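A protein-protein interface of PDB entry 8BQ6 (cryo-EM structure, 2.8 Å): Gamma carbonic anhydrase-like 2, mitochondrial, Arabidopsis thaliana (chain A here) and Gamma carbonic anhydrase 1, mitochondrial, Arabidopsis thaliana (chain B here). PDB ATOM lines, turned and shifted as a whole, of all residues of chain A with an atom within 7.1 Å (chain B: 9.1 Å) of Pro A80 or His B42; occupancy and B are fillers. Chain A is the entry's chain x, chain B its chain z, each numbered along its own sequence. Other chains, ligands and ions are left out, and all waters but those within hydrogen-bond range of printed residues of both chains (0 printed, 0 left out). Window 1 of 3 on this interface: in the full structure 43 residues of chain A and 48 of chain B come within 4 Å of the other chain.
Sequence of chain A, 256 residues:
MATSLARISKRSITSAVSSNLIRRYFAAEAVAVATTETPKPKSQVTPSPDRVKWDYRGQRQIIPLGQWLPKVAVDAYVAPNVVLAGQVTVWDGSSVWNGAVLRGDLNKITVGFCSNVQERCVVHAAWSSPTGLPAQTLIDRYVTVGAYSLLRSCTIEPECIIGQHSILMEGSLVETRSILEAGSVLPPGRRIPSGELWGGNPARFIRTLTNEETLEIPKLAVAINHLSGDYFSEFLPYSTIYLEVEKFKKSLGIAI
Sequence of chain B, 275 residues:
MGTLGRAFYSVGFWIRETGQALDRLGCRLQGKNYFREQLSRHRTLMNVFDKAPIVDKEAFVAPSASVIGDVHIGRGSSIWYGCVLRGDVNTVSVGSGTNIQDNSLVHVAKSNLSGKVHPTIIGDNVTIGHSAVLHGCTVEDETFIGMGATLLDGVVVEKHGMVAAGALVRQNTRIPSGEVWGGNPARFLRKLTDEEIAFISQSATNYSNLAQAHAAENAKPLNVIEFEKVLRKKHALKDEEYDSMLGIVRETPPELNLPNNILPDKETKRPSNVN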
ATOM      1  N   GLN A  59      30.623  19.243 -28.908  1.00  0.00           N
ATOM      2  CA  GLN A  59      31.129  19.600 -30.224  1.00  0.00           C
ATOM      3  C   GLN A  59      31.482  21.082 -30.248  1.00  0.00           C
ATOM      4  O   GLN A  59      30.671  21.924 -29.854  1.00  0.00           O
ATOM      5  CB  GLN A  59      30.093  19.274 -31.294  1.00  0.00           C
ATOM      6  CG  GLN A  59      30.414  19.847 -32.653  1.00  0.00           C
ATOM      7  CD  GLN A  59      31.599  19.168 -33.288  1.00  0.00           C
ATOM      8  OE1 GLN A  59      31.600  17.955 -33.472  1.00  0.00           O
ATOM      9  NE2 GLN A  59      32.615  19.945 -33.632  1.00  0.00           N
ATOM     10  N   ARG A  60      32.690  21.397 -30.706  1.00  0.00           N
ATOM     11  CA  ARG A  60      33.083  22.789 -30.871  1.00  0.00           C
ATOM     12  C   ARG A  60      32.301  23.425 -32.012  1.00  0.00           C
ATOM     13  O   ARG A  60      32.177  22.848 -33.095  1.00  0.00           O
ATOM     14  CB  ARG A  60      34.582  22.878 -31.139  1.00  0.00           C
ATOM     15  CG  ARG A  60      35.336  23.698 -30.124  1.00  0.00           C
ATOM     16  CD  ARG A  60      36.721  24.041 -30.615  1.00  0.00           C
ATOM     17  NE  ARG A  60      37.549  22.852 -30.775  1.00  0.00           N
ATOM     18  CZ  ARG A  60      38.628  22.793 -31.542  1.00  0.00           C
ATOM     19  NH1 ARG A  60      39.064  23.852 -32.204  1.00  0.00           N
ATOM     20  NH2 ARG A  60      39.289  21.644 -31.643  1.00  0.00           N
ATOM     21  N   GLN A  61      31.760  24.617 -31.760  1.00  0.00           N
ATOM     22  CA  GLN A  61      30.989  25.301 -32.789  1.00  0.00           C
ATOM     23  C   GLN A  61      31.875  25.763 -33.939  1.00  0.00           C
ATOM     24  O   GLN A  61      31.490  25.655 -35.110  1.00  0.00           O
ATOM     25  CB  GLN A  61      30.239  26.482 -32.184  1.00  0.00           C
ATOM     26  CG  GLN A  61      29.427  27.257 -33.191  1.00  0.00           C
ATOM     27  CD  GLN A  61      28.602  28.346 -32.554  1.00  0.00           C
ATOM     28  OE1 GLN A  61      29.081  29.451 -32.319  1.00  0.00           O
ATOM     29  NE2 GLN A  61      27.350  28.034 -32.266  1.00  0.00           N
ATOM     30  N   TYR A  77      23.587  35.921 -35.652  1.00  0.00           N
ATOM     31  CA  TYR A  77      23.176  34.882 -34.720  1.00  0.00           C
ATOM     32  C   TYR A  77      23.557  33.517 -35.270  1.00  0.00           C
ATOM     33  O   TYR A  77      23.182  33.167 -36.392  1.00  0.00           O
ATOM     34  CB  TYR A  77      21.675  34.917 -34.447  1.00  0.00           C
ATOM     35  CG  TYR A  77      21.230  33.747 -33.598  1.00  0.00           C
ATOM     36  CD1 TYR A  77      21.667  33.621 -32.291  1.00  0.00           C
ATOM     37  CD2 TYR A  77      20.393  32.762 -34.104  1.00  0.00           C
ATOM     38  CE1 TYR A  77      21.280  32.561 -31.507  1.00  0.00           C
ATOM     39  CE2 TYR A  77      19.997  31.692 -33.320  1.00  0.00           C
ATOM     40  CZ  TYR A  77      20.448  31.601 -32.020  1.00  0.00           C
ATOM     41  OH  TYR A  77      20.075  30.552 -31.216  1.00  0.00           O
ATOM     42  N   VAL A  78      24.284  32.746 -34.477  1.00  0.00           N
ATOM     43  CA  VAL A  78      24.583  31.361 -34.795  1.00  0.00           C
ATOM     44  C   VAL A  78      24.117  30.523 -33.615  1.00  0.00           C
ATOM     45  O   VAL A  78      24.461  30.820 -32.465  1.00  0.00           O
ATOM     46  CB  VAL A  78      26.077  31.149 -35.078  1.00  0.00           C
ATOM     47  CG1 VAL A  78      26.346  29.712 -35.439  1.00  0.00           C
ATOM     48  CG2 VAL A  78      26.538  32.077 -36.192  1.00  0.00           C
ATOM     49  N   ALA A  79      23.321  29.496 -33.897  1.00  0.00           N
ATOM     50  CA  ALA A  79      22.791  28.654 -32.840  1.00  0.00           C
ATOM     51  C   ALA A  79      23.927  27.889 -32.163  1.00  0.00           C
ATOM     52  O   ALA A  79      24.930  27.559 -32.803  1.00  0.00           O
ATOM     53  CB  ALA A  79      21.761  27.676 -33.396  1.00  0.00           C
ATOM     54  N   PRO A  80      23.792  27.590 -30.869  1.00  0.00           N
ATOM     55  CA  PRO A  80      24.903  26.941 -30.151  1.00  0.00           C
ATOM     56  C   PRO A  80      25.366  25.625 -30.758  1.00  0.00           C
ATOM     57  O   PRO A  80      26.564  25.326 -30.700  1.00  0.00           O
ATOM     58  CB  PRO A  80      24.330  26.747 -28.743  1.00  0.00           C
ATOM     59  CG  PRO A  80      23.321  27.814 -28.606  1.00  0.00           C
ATOM     60  CD  PRO A  80      22.704  27.984 -29.958  1.00  0.00           C
ATOM     61  N   ASN A  81      24.471  24.825 -31.336  1.00  0.00           N
ATOM     62  CA  ASN A  81      24.872  23.525 -31.860  1.00  0.00           C
ATOM     63  C   ASN A  81      25.106  23.529 -33.369  1.00  0.00           C
ATOM     64  O   ASN A  81      25.162  22.457 -33.978  1.00  0.00           O
ATOM     65  CB  ASN A  81      23.846  22.451 -31.478  1.00  0.00           C
ATOM     66  CG  ASN A  81      22.517  22.621 -32.181  1.00  0.00           C
ATOM     67  OD1 ASN A  81      22.170  23.706 -32.640  1.00  0.00           O
ATOM     68  ND2 ASN A  81      21.755  21.542 -32.250  1.00  0.00           N
ATOM     69  N   VAL A  82      25.255  24.705 -33.978  1.00  0.00           N
ATOM     70  CA  VAL A  82      25.706  24.787 -35.360  1.00  0.00           C
ATOM     71  C   VAL A  82      27.195  24.458 -35.426  1.00  0.00           C
ATOM     72  O   VAL A  82      27.966  24.773 -34.512  1.00  0.00           O
ATOM     73  CB  VAL A  82      25.415  26.190 -35.925  1.00  0.00           C
ATOM     74  CG1 VAL A  82      26.103  26.415 -37.264  1.00  0.00           C
ATOM     75  CG2 VAL A  82      23.925  26.407 -36.045  1.00  0.00           C
ATOM     76  N   VAL A  83      27.608  23.808 -36.510  1.00  0.00           N
ATOM     77  CA  VAL A  83      29.016  23.535 -36.776  1.00  0.00           C
ATOM     78  C   VAL A  83      29.436  24.359 -37.985  1.00  0.00           C
ATOM     79  O   VAL A  83      28.875  24.204 -39.076  1.00  0.00           O
ATOM     80  CB  VAL A  83      29.274  22.039 -37.009  1.00  0.00           C
ATOM     81  CG1 VAL A  83      30.702  21.810 -37.478  1.00  0.00           C
ATOM     82  CG2 VAL A  83      29.002  21.255 -35.740  1.00  0.00           C
ATOM     83  N   VAL A  96      22.105  31.550 -38.571  1.00  0.00           N
ATOM     84  CA  VAL A  96      22.190  30.113 -38.805  1.00  0.00           C
ATOM     85  C   VAL A  96      21.526  29.438 -37.614  1.00  0.00           C
ATOM     86  O   VAL A  96      21.866  29.736 -36.463  1.00  0.00           O
ATOM     87  CB  VAL A  96      23.646  29.636 -38.962  1.00  0.00           C
ATOM     88  CG1 VAL A  96      23.695  28.195 -39.429  1.00  0.00           C
ATOM     89  CG2 VAL A  96      24.403  30.534 -39.921  1.00  0.00           C
ATOM     90  N   TRP A  97      20.581  28.542 -37.881  1.00  0.00           N
ATOM     91  CA  TRP A  97      19.717  28.002 -36.842  1.00  0.00           C
ATOM     92  C   TRP A  97      20.090  26.562 -36.502  1.00  0.00           C
ATOM     93  O   TRP A  97      20.986  25.966 -37.101  1.00  0.00           O
ATOM     94  CB  TRP A  97      18.251  28.110 -37.272  1.00  0.00           C
ATOM     95  CG  TRP A  97      17.856  29.527 -37.476  1.00  0.00           C
ATOM     96  CD1 TRP A  97      18.206  30.322 -38.521  1.00  0.00           C
ATOM     97  CD2 TRP A  97      17.052  30.334 -36.608  1.00  0.00           C
ATOM     98  NE1 TRP A  97      17.671  31.573 -38.365  1.00  0.00           N
ATOM     99  CE2 TRP A  97      16.955  31.606 -37.199  1.00  0.00           C
ATOM    100  CE3 TRP A  97      16.402  30.104 -35.395  1.00  0.00           C
ATOM    101  CZ2 TRP A  97      16.235  32.645 -36.620  1.00  0.00           C
ATOM    102  CZ3 TRP A  97      15.687  31.138 -34.821  1.00  0.00           C
ATOM    103  CH2 TRP A  97      15.609  32.391 -35.434  1.00  0.00           C
ATOM    104  N   ASN A  98      19.364  26.005 -35.531  1.00  0.00           N
ATOM    105  CA  ASN A  98      19.773  24.782 -34.846  1.00  0.00           C
ATOM    106  C   ASN A  98      19.991  23.619 -35.800  1.00  0.00           C
ATOM    107  O   ASN A  98      19.166  23.345 -36.673  1.00  0.00           O
ATOM    108  CB  ASN A  98      18.722  24.388 -33.809  1.00  0.00           C
ATOM    109  CG  ASN A  98      18.543  25.431 -32.749  1.00  0.00           C
ATOM    110  OD1 ASN A  98      18.019  26.511 -33.007  1.00  0.00           O
ATOM    111  ND2 ASN A  98      18.989  25.122 -31.540  1.00  0.00           N
ATOM    112  N   GLY A  99      21.102  22.916 -35.599  1.00  0.00           N
ATOM    113  CA  GLY A  99      21.384  21.707 -36.333  1.00  0.00           C
ATOM    114  C   GLY A  99      22.005  21.902 -37.695  1.00  0.00           C
ATOM    115  O   GLY A  99      22.290  20.907 -38.369  1.00  0.00           O
ATOM    116  N   TYR A 231      16.793  35.564 -30.034  1.00  0.00           N
ATOM    117  CA  TYR A 231      17.672  34.470 -29.630  1.00  0.00           C
ATOM    118  C   TYR A 231      19.075  34.972 -29.326  1.00  0.00           C
ATOM    119  O   TYR A 231      19.755  34.443 -28.440  1.00  0.00           O
ATOM    120  CB  TYR A 231      17.714  33.407 -30.722  1.00  0.00           C
ATOM    121  CG  TYR A 231      16.477  32.559 -30.782  1.00  0.00           C
ATOM    122  CD1 TYR A 231      15.309  33.039 -31.354  1.00  0.00           C
ATOM    123  CD2 TYR A 231      16.475  31.277 -30.267  1.00  0.00           C
ATOM    124  CE1 TYR A 231      14.178  32.264 -31.407  1.00  0.00           C
ATOM    125  CE2 TYR A 231      15.354  30.497 -30.318  1.00  0.00           C
ATOM    126  CZ  TYR A 231      14.207  30.990 -30.888  1.00  0.00           C
ATOM    127  OH  TYR A 231      13.083  30.201 -30.936  1.00  0.00           O
ATOM    128  N   PHE A 235      21.992  35.211 -24.933  1.00  0.00           N
ATOM    129  CA  PHE A 235      23.327  34.683 -24.671  1.00  0.00           C
ATOM    130  C   PHE A 235      24.270  35.814 -24.288  1.00  0.00           C
ATOM    131  O   PHE A 235      24.446  36.769 -25.053  1.00  0.00           O
ATOM    132  CB  PHE A 235      23.853  33.933 -25.895  1.00  0.00           C
ATOM    133  CG  PHE A 235      23.155  32.632 -26.141  1.00  0.00           C
ATOM    134  CD1 PHE A 235      23.515  31.495 -25.443  1.00  0.00           C
ATOM    135  CD2 PHE A 235      22.108  32.558 -27.039  1.00  0.00           C
ATOM    136  CE1 PHE A 235      22.862  30.304 -25.660  1.00  0.00           C
ATOM    137  CE2 PHE A 235      21.450  31.369 -27.258  1.00  0.00           C
ATOM    138  CZ  PHE A 235      21.827  30.243 -26.569  1.00  0.00           C
ATOM    139  N   ILE A 241      29.739  27.460 -18.068  1.00  0.00           N
ATOM    140  CA  ILE A 241      30.035  26.029 -18.021  1.00  0.00           C
ATOM    141  C   ILE A 241      31.351  25.778 -17.302  1.00  0.00           C
ATOM    142  O   ILE A 241      31.515  24.762 -16.614  1.00  0.00           O
ATOM    143  CB  ILE A 241      30.065  25.437 -19.442  1.00  0.00           C
ATOM    144  CG1 ILE A 241      28.766  25.722 -20.172  1.00  0.00           C
ATOM    145  CG2 ILE A 241      30.253  23.937 -19.383  1.00  0.00           C
ATOM    146  CD1 ILE A 241      27.617  25.109 -19.512  1.00  0.00           C
ATOM    147  N   LEU B  39      33.324  25.686 -24.658  1.00  0.00           N
ATOM    148  CA  LEU B  39      32.439  24.598 -24.278  1.00  0.00           C
ATOM    149  C   LEU B  39      31.065  24.827 -24.890  1.00  0.00           C
ATOM    150  O   LEU B  39      30.651  25.971 -25.101  1.00  0.00           O
ATOM    151  CB  LEU B  39      32.335  24.471 -22.754  1.00  0.00           C
ATOM    152  CG  LEU B  39      33.650  24.291 -21.984  1.00  0.00           C
ATOM    153  CD1 LEU B  39      33.634  25.061 -20.673  1.00  0.00           C
ATOM    154  CD2 LEU B  39      33.957  22.819 -21.740  1.00  0.00           C
ATOM    155  N   SER B  40      30.369  23.735 -25.190  1.00  0.00           N
ATOM    156  CA  SER B  40      29.116  23.837 -25.919  1.00  0.00           C
ATOM    157  C   SER B  40      28.047  24.498 -25.065  1.00  0.00           C
ATOM    158  O   SER B  40      27.828  24.122 -23.910  1.00  0.00           O
ATOM    159  CB  SER B  40      28.644  22.458 -26.370  1.00  0.00           C
ATOM    160  OG  SER B  40      27.473  22.573 -27.160  1.00  0.00           O
ATOM    161  N   ARG B  41      27.373  25.482 -25.645  1.00  0.00           N
ATOM    162  CA  ARG B  41      26.291  26.173 -24.973  1.00  0.00           C
ATOM    163  C   ARG B  41      24.933  25.602 -25.350  1.00  0.00           C
ATOM    164  O   ARG B  41      23.909  26.232 -25.078  1.00  0.00           O
ATOM    165  CB  ARG B  41      26.367  27.668 -25.282  1.00  0.00           C
ATOM    166  CG  ARG B  41      27.776  28.223 -25.119  1.00  0.00           C
ATOM    167  CD  ARG B  41      27.811  29.731 -25.204  1.00  0.00           C
ATOM    168  NE  ARG B  41      27.022  30.361 -24.155  1.00  0.00           N
ATOM    169  CZ  ARG B  41      27.038  31.660 -23.893  1.00  0.00           C
ATOM    170  NH1 ARG B  41      27.801  32.493 -24.579  1.00  0.00           N
ATOM    171  NH2 ARG B  41      26.267  32.136 -22.920  1.00  0.00           N
ATOM    172  N   HIS B  42      24.910  24.421 -25.965  1.00  0.00           N
ATOM    173  CA  HIS B  42      23.649  23.797 -26.335  1.00  0.00           C
ATOM    174  C   HIS B  42      22.846  23.443 -25.093  1.00  0.00           C
ATOM    175  O   HIS B  42      23.362  22.836 -24.151  1.00  0.00           O
ATOM    176  CB  HIS B  42      23.891  22.540 -27.166  1.00  0.00           C
ATOM    177  CG  HIS B  42      22.677  21.676 -27.305  1.00  0.00           C
ATOM    178  ND1 HIS B  42      21.647  21.978 -28.170  1.00  0.00           N
ATOM    179  CD2 HIS B  42      22.312  20.539 -26.668  1.00  0.00           C
ATOM    180  CE1 HIS B  42      20.709  21.054 -28.073  1.00  0.00           C
ATOM    181  NE2 HIS B  42      21.086  20.169 -27.168  1.00  0.00           N
ATOM    182  N   ARG B  43      21.575  23.822 -25.102  1.00  0.00           N
ATOM    183  CA  ARG B  43      20.637  23.465 -24.052  1.00  0.00           C
ATOM    184  C   ARG B  43      19.568  22.572 -24.657  1.00  0.00           C
ATOM    185  O   ARG B  43      18.979  22.917 -25.686  1.00  0.00           O
ATOM    186  CB  ARG B  43      20.005  24.708 -23.425  1.00  0.00           C
ATOM    187  CG  ARG B  43      20.909  25.438 -22.455  1.00  0.00           C
ATOM    188  CD  ARG B  43      20.298  26.745 -22.000  1.00  0.00           C
ATOM    189  NE  ARG B  43      20.223  27.723 -23.078  1.00  0.00           N
ATOM    190  CZ  ARG B  43      19.536  28.855 -23.014  1.00  0.00           C
ATOM    191  NH1 ARG B  43      18.856  29.190 -21.929  1.00  0.00           N
ATOM    192  NH2 ARG B  43      19.538  29.675 -24.060  1.00  0.00           N
ATOM    193  N   THR B  44      19.333  21.423 -24.028  1.00  0.00           N
ATOM    194  CA  THR B  44      18.275  20.536 -24.495  1.00  0.00           C
ATOM    195  C   THR B  44      16.919  21.227 -24.424  1.00  0.00           C
ATOM    196  O   THR B  44      16.103  21.113 -25.346  1.00  0.00           O
ATOM    197  CB  THR B  44      18.279  19.255 -23.663  1.00  0.00           C
ATOM    198  OG1 THR B  44      19.610  18.731 -23.614  1.00  0.00           O
ATOM    199  CG2 THR B  44      17.375  18.221 -24.272  1.00  0.00           C
ATOM    200  N   LEU B  45      16.670  21.956 -23.343  1.00  0.00           N
ATOM    201  CA  LEU B  45      15.465  22.749 -23.171  1.00  0.00           C
ATOM    202  C   LEU B  45      15.859  24.214 -23.105  1.00  0.00           C
ATOM    203  O   LEU B  45      16.572  24.627 -22.186  1.00  0.00           O
ATOM    204  CB  LEU B  45      14.722  22.337 -21.902  1.00  0.00           C
ATOM    205  CG  LEU B  45      14.529  20.831 -21.733  1.00  0.00           C
ATOM    206  CD1 LEU B  45      13.797  20.548 -20.440  1.00  0.00           C
ATOM    207  CD2 LEU B  45      13.771  20.256 -22.914  1.00  0.00           C
ATOM    208  N   MET B  46      15.404  24.993 -24.078  1.00  0.00           N
ATOM    209  CA  MET B  46      15.781  26.393 -24.174  1.00  0.00           C
ATOM    210  C   MET B  46      14.541  27.260 -24.058  1.00  0.00           C
ATOM    211  O   MET B  46      13.523  26.986 -24.701  1.00  0.00           O
ATOM    212  CB  MET B  46      16.504  26.686 -25.487  1.00  0.00           C
ATOM    213  CG  MET B  46      17.191  28.030 -25.505  1.00  0.00           C
ATOM    214  SD  MET B  46      17.963  28.417 -27.084  1.00  0.00           S
ATOM    215  CE  MET B  46      17.687  30.183 -27.162  1.00  0.00           C
ATOM    216  N   VAL B  61      13.842  12.525 -23.723  1.00  0.00           N
ATOM    217  CA  VAL B  61      14.376  13.530 -24.630  1.00  0.00           C
ATOM    218  C   VAL B  61      15.864  13.261 -24.777  1.00  0.00           C
ATOM    219  O   VAL B  61      16.595  13.256 -23.781  1.00  0.00           O
ATOM    220  CB  VAL B  61      14.135  14.960 -24.125  1.00  0.00           C
ATOM    221  CG1 VAL B  61      14.795  15.951 -25.052  1.00  0.00           C
ATOM    222  CG2 VAL B  61      12.648  15.247 -24.009  1.00  0.00           C
ATOM    223  N   ALA B  62      16.309  13.039 -26.005  1.00  0.00           N
ATOM    224  CA  ALA B  62      17.730  12.845 -26.235  1.00  0.00           C
ATOM    225  C   ALA B  62      18.482  14.132 -25.902  1.00  0.00           C
ATOM    226  O   ALA B  62      17.979  15.231 -26.159  1.00  0.00           O
ATOM    227  CB  ALA B  62      17.987  12.434 -27.682  1.00  0.00           C
ATOM    228  N   PRO B  63      19.671  14.034 -25.301  1.00  0.00           N
ATOM    229  CA  PRO B  63      20.402  15.258 -24.923  1.00  0.00           C
ATOM    230  C   PRO B  63      20.740  16.169 -26.089  1.00  0.00           C
ATOM    231  O   PRO B  63      20.781  17.392 -25.913  1.00  0.00           O
ATOM    232  CB  PRO B  63      21.665  14.709 -24.249  1.00  0.00           C
ATOM    233  CG  PRO B  63      21.280  13.361 -23.770  1.00  0.00           C
ATOM    234  CD  PRO B  63      20.289  12.820 -24.747  1.00  0.00           C
ATOM    235  N   SER B  64      20.991  15.612 -27.274  1.00  0.00           N
ATOM    236  CA  SER B  64      21.361  16.419 -28.430  1.00  0.00           C
ATOM    237  C   SER B  64      20.157  17.020 -29.142  1.00  0.00           C
ATOM    238  O   SER B  64      20.339  17.773 -30.104  1.00  0.00           O
ATOM    239  CB  SER B  64      22.181  15.583 -29.417  1.00  0.00           C
ATOM    240  OG  SER B  64      21.399  14.565 -30.017  1.00  0.00           O
ATOM    241  N   ALA B  65      18.944  16.705 -28.697  1.00  0.00           N
ATOM    242  CA  ALA B  65      17.745  17.293 -29.271  1.00  0.00           C
ATOM    243  C   ALA B  65      17.577  18.734 -28.798  1.00  0.00           C
ATOM    244  O   ALA B  65      18.067  19.123 -27.737  1.00  0.00           O
ATOM    245  CB  ALA B  65      16.521  16.463 -28.888  1.00  0.00           C
ATOM    246  N   SER B  66      16.880  19.534 -29.603  1.00  0.00           N
ATOM    247  CA  SER B  66      16.643  20.942 -29.301  1.00  0.00           C
ATOM    248  C   SER B  66      15.153  21.176 -29.118  1.00  0.00           C
ATOM    249  O   SER B  66      14.367  20.954 -30.044  1.00  0.00           O
ATOM    250  CB  SER B  66      17.181  21.853 -30.406  1.00  0.00           C
ATOM    251  OG  SER B  66      18.571  21.681 -30.603  1.00  0.00           O
ATOM    252  N   VAL B  67      14.770  21.641 -27.935  1.00  0.00           N
ATOM    253  CA  VAL B  67      13.386  21.962 -27.620  1.00  0.00           C
ATOM    254  C   VAL B  67      13.357  23.416 -27.177  1.00  0.00           C
ATOM    255  O   VAL B  67      13.804  23.744 -26.071  1.00  0.00           O
ATOM    256  CB  VAL B  67      12.816  21.032 -26.544  1.00  0.00           C
ATOM    257  CG1 VAL B  67      11.366  21.339 -26.312  1.00  0.00           C
ATOM    258  CG2 VAL B  67      12.983  19.579 -26.962  1.00  0.00           C
ATOM    259  N   ILE B  68      12.832  24.289 -28.032  1.00  0.00           N
ATOM    260  CA  ILE B  68      12.970  25.730 -27.865  1.00  0.00           C
ATOM    261  C   ILE B  68      11.597  26.360 -27.712  1.00  0.00           C
ATOM    262  O   ILE B  68      10.717  26.164 -28.558  1.00  0.00           O
ATOM    263  CB  ILE B  68      13.717  26.370 -29.047  1.00  0.00           C
ATOM    264  CG1 ILE B  68      14.985  25.585 -29.377  1.00  0.00           C
ATOM    265  CG2 ILE B  68      14.055  27.799 -28.726  1.00  0.00           C
ATOM    266  CD1 ILE B  68      15.083  25.183 -30.831  1.00  0.00           C
ATOM    267  N   GLY B  82      18.987  14.299 -32.248  1.00  0.00           N
ATOM    268  CA  GLY B  82      19.089  15.295 -33.291  1.00  0.00           C
ATOM    269  C   GLY B  82      17.808  16.016 -33.644  1.00  0.00           C
ATOM    270  O   GLY B  82      17.822  16.841 -34.565  1.00  0.00           O
ATOM    271  N   CYS B  83      16.707  15.744 -32.952  1.00  0.00           N
ATOM    272  CA  CYS B  83      15.450  16.405 -33.272  1.00  0.00           C
ATOM    273  C   CYS B  83      15.492  17.875 -32.876  1.00  0.00           C
ATOM    274  O   CYS B  83      16.253  18.287 -31.999  1.00  0.00           O
ATOM    275  CB  CYS B  83      14.287  15.721 -32.561  1.00  0.00           C
ATOM    276  SG  CYS B  83      13.921  14.088 -33.164  1.00  0.00           S
ATOM    277  N   VAL B  84      14.666  18.671 -33.545  1.00  0.00           N
ATOM    278  CA  VAL B  84      14.521  20.087 -33.246  1.00  0.00           C
ATOM    279  C   VAL B  84      13.037  20.402 -33.160  1.00  0.00           C
ATOM    280  O   VAL B  84      12.279  20.086 -34.084  1.00  0.00           O
ATOM    281  CB  VAL B  84      15.205  20.970 -34.308  1.00  0.00           C
ATOM    282  CG1 VAL B  84      14.943  22.432 -34.023  1.00  0.00           C
ATOM    283  CG2 VAL B  84      16.702  20.692 -34.353  1.00  0.00           C
ATOM    284  N   LEU B  85      12.619  21.012 -32.054  1.00  0.00           N
ATOM    285  CA  LEU B  85      11.248  21.486 -31.897  1.00  0.00           C
ATOM    286  C   LEU B  85      11.289  22.939 -31.463  1.00  0.00           C
ATOM    287  O   LEU B  85      11.769  23.247 -30.368  1.00  0.00           O
ATOM    288  CB  LEU B  85      10.466  20.647 -30.885  1.00  0.00           C
ATOM    289  CG  LEU B  85      10.142  19.212 -31.290  1.00  0.00           C
ATOM    290  CD1 LEU B  85      11.238  18.285 -30.821  1.00  0.00           C
ATOM    291  CD2 LEU B  85       8.805  18.787 -30.712  1.00  0.00           C
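O of Pro A80 lies within hydrogen-bond range of NE2 of Gln A61.
OD1 of Asn A81 is in hydrogen-bond range of N of Gly A99 (3.2 Å).
A ring nitrogen (NE2) of His B42 sits at hydrogen-bond distance from the backbone carbonyl oxygen (O) of Pro B63 (3.1 Å).
The backbone NH of Ser B66 lies within hydrogen-bond range of the backbone carbonyl oxygen of Cys B83 (2.8 Å).
O of Ser B66 sits at hydrogen-bond distance from N of Leu B85.
The backbone NH (N) of Ile B68 lies within hydrogen-bond range of the backbone carbonyl oxygen (O) of Leu B85, at 2.8 Å.
Pro A80 touches Arg B41.
N of His B42 touches CB of Pro A80, at 3.7 Å.
Asn A98 touches Ser B66.
OD1 of Asn A98 touches CD1 of Ile B68 (3.9 Å).
CD2 of Tyr A231 touches CE of Met B46, at 3.5 Å.
Tyr A231 touches Ile B68.
Phe A235 touches Arg B41 (CD1 to NH2, 3.8 Å).
Phe A235 touches Arg B43.
CE2 of Phe A235 touches CE of Met B46, 3.9 Å away.
Ile A241 touches Leu B39 (CG2 to CD1, 3.8 Å).
Of chain B, only Arg B41 (3.6 Å) and His B42 (3.7 Å) come within 4 Å of Pro A80.
Printed residues of chain A within 4 Å of His B42: Pro A80 (3.7 Å).
No residue of chain B comes within 4 Å of Ala A79.
Of the printed residues of chain A, Arg B43 touches Phe A235 (3.4 Å).
Of the printed residues of chain A, Arg B41 touches Pro A80 (3.6 Å) and Phe A235 (3.8 Å).
The nearest printed residue of chain A that does not touch His B42 is Asn A81 (4.0003 Å).
Among the printed residues, 11 pairs touch across the chains.
Among the printed residues, no Asp or Glu carboxylate lies within 4 Å of a Lys or Arg side-chain nitrogen of the other chain.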
